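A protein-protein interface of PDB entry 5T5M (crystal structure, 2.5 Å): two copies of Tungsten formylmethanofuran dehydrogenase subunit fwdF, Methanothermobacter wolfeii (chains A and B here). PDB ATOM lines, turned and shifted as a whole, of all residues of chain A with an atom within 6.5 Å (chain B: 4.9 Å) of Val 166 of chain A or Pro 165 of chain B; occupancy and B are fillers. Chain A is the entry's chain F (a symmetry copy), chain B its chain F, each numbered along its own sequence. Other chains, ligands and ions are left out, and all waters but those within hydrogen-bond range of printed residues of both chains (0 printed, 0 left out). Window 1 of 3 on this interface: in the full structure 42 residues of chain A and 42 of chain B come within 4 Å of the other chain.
The side-chain sulfur (SG) of Cys 164 of chain B lies close to the backbone NH (N) of Val 166 of chain B.
The side-chain sulfur (SG) of Cys 197 of chain B lies close to the backbone NH (N) of Ile 199 of chain B (3.4 Å).
The guanidinium group (NH1) of Arg 139 of chain A is in hydrogen-bond range of the backbone carbonyl oxygen (O) of Lys 193 of chain A.
N of Val 166 of chain A lies close to SG of Cys 164 of chain A (3.5 Å).
Pro 165 of chain B touches Arg 139 of chain A.
CG of Arg 139 of chain A touches CD1 of Ile 199 of chain B, 3.5 Å away.
CB of Pro 165 of chain A touches CG1 of Val 166 of chain B, at 3.7 Å.
CG1 of Val 166 of chain A touches CB of Pro 165 of chain B (3.7 Å).
CB of Pro 165 of chain B touches CG1 of Val 195 of chain A, at 3.9 Å.
Cys 197 of chain B touches Val 195 of chain A.
Ile 199 of chain B touches Val 195 of chain A (CD1 to CG1, 3.99 Å).
Pro 165 of chain B touches three residues of chain A.
Of the printed residues of chain A, Cys 197 of chain B touches Val 195 (3.4 Å).
Of the printed residues of chain A, Val 166 of chain B touches Pro 165 (3.7 Å).
Printed residues of chain B within 4 Å of Pro 165 of chain A: Val 166 (3.7 Å).
Asp 167 of chain B touches none of the printed residues of chain A.
Cys 194 of chain A touches none of the printed residues of chain B.
The nearest residue of chain B that does not touch Val 166 of chain A is Val 166 of chain B (4.6 Å).
Among the printed residues, 7 pairs touch across the chains.
Pro 165 of chain A touches Val 166 of chain B, and with the chains exchanged Val 166 of chain A touches Pro 165 of chain B.
Of the 7 pairs that touch across the chains among the printed residues, 2 have their exchanged pair printed and touching as well.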
ATOM      1  N   ARG A 139     -27.035  18.343 -13.169  1.00  0.00           N
ATOM      2  CA  ARG A 139     -25.775  19.000 -13.498  1.00  0.00           C
ATOM      3  C   ARG A 139     -25.994  20.221 -14.381  1.00  0.00           C
ATOM      4  O   ARG A 139     -25.420  21.286 -14.134  1.00  0.00           O
ATOM      5  CB  ARG A 139     -24.843  18.013 -14.190  1.00  0.00           C
ATOM      6  CG  ARG A 139     -23.384  18.420 -14.171  1.00  0.00           C
ATOM      7  CD  ARG A 139     -22.487  17.247 -14.526  1.00  0.00           C
ATOM      8  NE  ARG A 139     -22.348  17.071 -15.967  1.00  0.00           N
ATOM      9  CZ  ARG A 139     -21.758  16.025 -16.533  1.00  0.00           C
ATOM     10  NH1 ARG A 139     -21.661  15.947 -17.856  1.00  0.00           N
ATOM     11  NH2 ARG A 139     -21.267  15.051 -15.779  1.00  0.00           N
ATOM     12  N   MET A 163     -11.259  15.521 -26.812  1.00  0.00           N
ATOM     13  CA  MET A 163     -10.845  16.275 -25.641  1.00  0.00           C
ATOM     14  C   MET A 163     -11.995  16.644 -24.708  1.00  0.00           C
ATOM     15  O   MET A 163     -11.736  17.072 -23.584  1.00  0.00           O
ATOM     16  CB  MET A 163     -10.123  17.549 -26.087  1.00  0.00           C
ATOM     17  CG  MET A 163      -8.860  17.289 -26.873  1.00  0.00           C
ATOM     18  SD  MET A 163      -7.493  16.786 -25.821  1.00  0.00           S
ATOM     19  CE  MET A 163      -6.874  18.388 -25.303  1.00  0.00           C
ATOM     20  N   CYS A 164     -13.245  16.509 -25.135  1.00  0.00           N
ATOM     21  CA  CYS A 164     -14.346  16.895 -24.267  1.00  0.00           C
ATOM     22  C   CYS A 164     -14.277  16.047 -22.999  1.00  0.00           C
ATOM     23  O   CYS A 164     -14.283  14.810 -23.091  1.00  0.00           O
ATOM     24  CB  CYS A 164     -15.698  16.716 -24.951  1.00  0.00           C
ATOM     25  SG  CYS A 164     -17.148  17.048 -23.846  1.00  0.00           S
ATOM     26  N   PRO A 165     -14.188  16.654 -21.813  1.00  0.00           N
ATOM     27  CA  PRO A 165     -14.030  15.846 -20.598  1.00  0.00           C
ATOM     28  C   PRO A 165     -15.283  15.095 -20.207  1.00  0.00           C
ATOM     29  O   PRO A 165     -15.214  14.268 -19.295  1.00  0.00           O
ATOM     30  CB  PRO A 165     -13.645  16.884 -19.537  1.00  0.00           C
ATOM     31  CG  PRO A 165     -14.254  18.157 -20.023  1.00  0.00           C
ATOM     32  CD  PRO A 165     -14.202  18.097 -21.516  1.00  0.00           C
ATOM     33  N   VAL A 166     -16.413  15.334 -20.869  1.00  0.00           N
ATOM     34  CA  VAL A 166     -17.677  14.739 -20.456  1.00  0.00           C
ATOM     35  C   VAL A 166     -18.397  14.101 -21.635  1.00  0.00           C
ATOM     36  O   VAL A 166     -19.575  13.759 -21.534  1.00  0.00           O
ATOM     37  CB  VAL A 166     -18.569  15.795 -19.787  1.00  0.00           C
ATOM     38  CG1 VAL A 166     -17.964  16.225 -18.465  1.00  0.00           C
ATOM     39  CG2 VAL A 166     -18.755  16.997 -20.710  1.00  0.00           C
ATOM     40  N   ASP A 167     -17.694  13.935 -22.756  1.00  0.00           N
ATOM     41  CA  ASP A 167     -18.237  13.297 -23.955  1.00  0.00           C
ATOM     42  C   ASP A 167     -19.573  13.918 -24.372  1.00  0.00           C
ATOM     43  O   ASP A 167     -20.544  13.226 -24.690  1.00  0.00           O
ATOM     44  CB  ASP A 167     -18.357  11.790 -23.748  1.00  0.00           C
ATOM     45  CG  ASP A 167     -16.993  11.116 -23.560  1.00  0.00           C
ATOM     46  OD1 ASP A 167     -15.969  11.641 -24.066  1.00  0.00           O
ATOM     47  OD2 ASP A 167     -16.944  10.052 -22.909  1.00  0.00           O
ATOM     48  N   ALA A 168     -19.602  15.251 -24.404  1.00  0.00           N
ATOM     49  CA  ALA A 168     -20.781  15.980 -24.850  1.00  0.00           C
ATOM     50  C   ALA A 168     -20.824  16.215 -26.360  1.00  0.00           C
ATOM     51  O   ALA A 168     -21.900  16.521 -26.893  1.00  0.00           O
ATOM     52  CB  ALA A 168     -20.860  17.334 -24.134  1.00  0.00           C
ATOM     53  N   ILE A 169     -19.698  16.090 -27.059  1.00  0.00           N
ATOM     54  CA  ILE A 169     -19.652  16.315 -28.500  1.00  0.00           C
ATOM     55  C   ILE A 169     -19.658  14.971 -29.214  1.00  0.00           C
ATOM     56  O   ILE A 169     -18.871  14.074 -28.881  1.00  0.00           O
ATOM     57  CB  ILE A 169     -18.416  17.133 -28.912  1.00  0.00           C
ATOM     58  CG1 ILE A 169     -18.478  18.532 -28.308  1.00  0.00           C
ATOM     59  CG2 ILE A 169     -18.352  17.248 -30.420  1.00  0.00           C
ATOM     60  CD1 ILE A 169     -17.182  19.296 -28.404  1.00  0.00           C
ATOM     61  N   LYS A 193     -25.046  17.514 -21.052  1.00  0.00           N
ATOM     62  CA  LYS A 193     -23.778  17.023 -20.524  1.00  0.00           C
ATOM     63  C   LYS A 193     -22.721  18.110 -20.419  1.00  0.00           C
ATOM     64  O   LYS A 193     -21.867  18.052 -19.528  1.00  0.00           O
ATOM     65  CB  LYS A 193     -23.237  15.894 -21.417  1.00  0.00           C
ATOM     66  CG  LYS A 193     -24.153  14.694 -21.516  1.00  0.00           C
ATOM     67  CD  LYS A 193     -23.513  13.576 -22.308  1.00  0.00           C
ATOM     68  CE  LYS A 193     -24.448  12.385 -22.439  1.00  0.00           C
ATOM     69  NZ  LYS A 193     -23.961  11.424 -23.469  1.00  0.00           N
ATOM     70  N   CYS A 194     -22.769  19.093 -21.310  1.00  0.00           N
ATOM     71  CA  CYS A 194     -21.741  20.120 -21.382  1.00  0.00           C
ATOM     72  C   CYS A 194     -21.631  20.876 -20.056  1.00  0.00           C
ATOM     73  O   CYS A 194     -22.638  21.287 -19.474  1.00  0.00           O
ATOM     74  CB  CYS A 194     -22.079  21.057 -22.547  1.00  0.00           C
ATOM     75  SG  CYS A 194     -21.181  22.608 -22.684  1.00  0.00           S
ATOM     76  N   VAL A 195     -20.401  21.045 -19.572  1.00  0.00           N
ATOM     77  CA  VAL A 195     -20.136  21.777 -18.330  1.00  0.00           C
ATOM     78  C   VAL A 195     -19.409  23.087 -18.600  1.00  0.00           C
ATOM     79  O   VAL A 195     -18.918  23.729 -17.657  1.00  0.00           O
ATOM     80  CB  VAL A 195     -19.351  20.920 -17.321  1.00  0.00           C
ATOM     81  CG1 VAL A 195     -20.128  19.666 -16.962  1.00  0.00           C
ATOM     82  CG2 VAL A 195     -17.996  20.549 -17.884  1.00  0.00           C
ATOM     83  N   MET B 163     -20.822  15.355  -7.653  1.00  0.00           N
ATOM     84  CA  MET B 163     -21.196  16.178  -8.789  1.00  0.00           C
ATOM     85  C   MET B 163     -20.028  16.528  -9.707  1.00  0.00           C
ATOM     86  O   MET B 163     -20.263  17.017 -10.812  1.00  0.00           O
ATOM     87  CB  MET B 163     -21.853  17.468  -8.289  1.00  0.00           C
ATOM     88  CG  MET B 163     -23.127  17.239  -7.514  1.00  0.00           C
ATOM     89  SD  MET B 163     -24.517  16.853  -8.584  1.00  0.00           S
ATOM     90  CE  MET B 163     -25.053  18.504  -9.032  1.00  0.00           C
ATOM     91  N   CYS B 164     -18.786  16.311  -9.288  1.00  0.00           N
ATOM     92  CA  CYS B 164     -17.666  16.678 -10.140  1.00  0.00           C
ATOM     93  C   CYS B 164     -17.778  15.889 -11.443  1.00  0.00           C
ATOM     94  O   CYS B 164     -17.835  14.650 -11.404  1.00  0.00           O
ATOM     95  CB  CYS B 164     -16.326  16.399  -9.465  1.00  0.00           C
ATOM     96  SG  CYS B 164     -14.859  16.705 -10.556  1.00  0.00           S
ATOM     97  N   PRO B 165     -17.834  16.550 -12.602  1.00  0.00           N
ATOM     98  CA  PRO B 165     -18.032  15.804 -13.850  1.00  0.00           C
ATOM     99  C   PRO B 165     -16.818  15.006 -14.274  1.00  0.00           C
ATOM    100  O   PRO B 165     -16.929  14.224 -15.221  1.00  0.00           O
ATOM    101  CB  PRO B 165     -18.361  16.904 -14.865  1.00  0.00           C
ATOM    102  CG  PRO B 165     -17.689  18.123 -14.325  1.00  0.00           C
ATOM    103  CD  PRO B 165     -17.745  18.002 -12.837  1.00  0.00           C
ATOM    104  N   VAL B 166     -15.678  15.160 -13.604  1.00  0.00           N
ATOM    105  CA  VAL B 166     -14.446  14.518 -14.043  1.00  0.00           C
ATOM    106  C   VAL B 166     -13.761  13.795 -12.893  1.00  0.00           C
ATOM    107  O   VAL B 166     -12.601  13.398 -13.011  1.00  0.00           O
ATOM    108  CB  VAL B 166     -13.500  15.555 -14.667  1.00  0.00           C
ATOM    109  CG1 VAL B 166     -14.081  16.072 -15.969  1.00  0.00           C
ATOM    110  CG2 VAL B 166     -13.254  16.706 -13.694  1.00  0.00           C
ATOM    111  N   ASP B 167     -14.473  13.618 -11.780  1.00  0.00           N
ATOM    112  CA  ASP B 167     -13.964  12.902 -10.610  1.00  0.00           C
ATOM    113  C   ASP B 167     -12.599  13.435 -10.168  1.00  0.00           C
ATOM    114  O   ASP B 167     -11.665  12.681  -9.881  1.00  0.00           O
ATOM    115  CB  ASP B 167     -13.921  11.401 -10.881  1.00  0.00           C
ATOM    116  CG  ASP B 167     -15.318  10.806 -11.096  1.00  0.00           C
ATOM    117  OD1 ASP B 167     -16.315  11.361 -10.567  1.00  0.00           O
ATOM    118  OD2 ASP B 167     -15.420   9.775 -11.793  1.00  0.00           O
ATOM    119  N   CYS B 197     -15.096  24.059 -14.093  1.00  0.00           N
ATOM    120  CA  CYS B 197     -16.480  24.356 -14.408  1.00  0.00           C
ATOM    121  C   CYS B 197     -17.226  25.022 -13.264  1.00  0.00           C
ATOM    122  O   CYS B 197     -18.336  25.516 -13.484  1.00  0.00           O
ATOM    123  CB  CYS B 197     -17.216  23.070 -14.792  1.00  0.00           C
ATOM    124  SG  CYS B 197     -17.601  21.997 -13.385  1.00  0.00           S
ATOM    125  N   ILE B 199     -18.854  23.815 -10.773  1.00  0.00           N
ATOM    126  CA  ILE B 199     -20.020  23.120 -10.232  1.00  0.00           C
ATOM    127  C   ILE B 199     -19.868  22.915  -8.729  1.00  0.00           C
ATOM    128  O   ILE B 199     -20.814  23.110  -7.957  1.00  0.00           O
ATOM    129  CB  ILE B 199     -20.226  21.777 -10.956  1.00  0.00           C
ATOM    130  CG1 ILE B 199     -20.844  22.010 -12.339  1.00  0.00           C
ATOM    131  CG2 ILE B 199     -21.111  20.830 -10.110  1.00  0.00           C
ATOM    132  CD1 ILE B 199     -20.911  20.764 -13.210  1.00  0.00           C
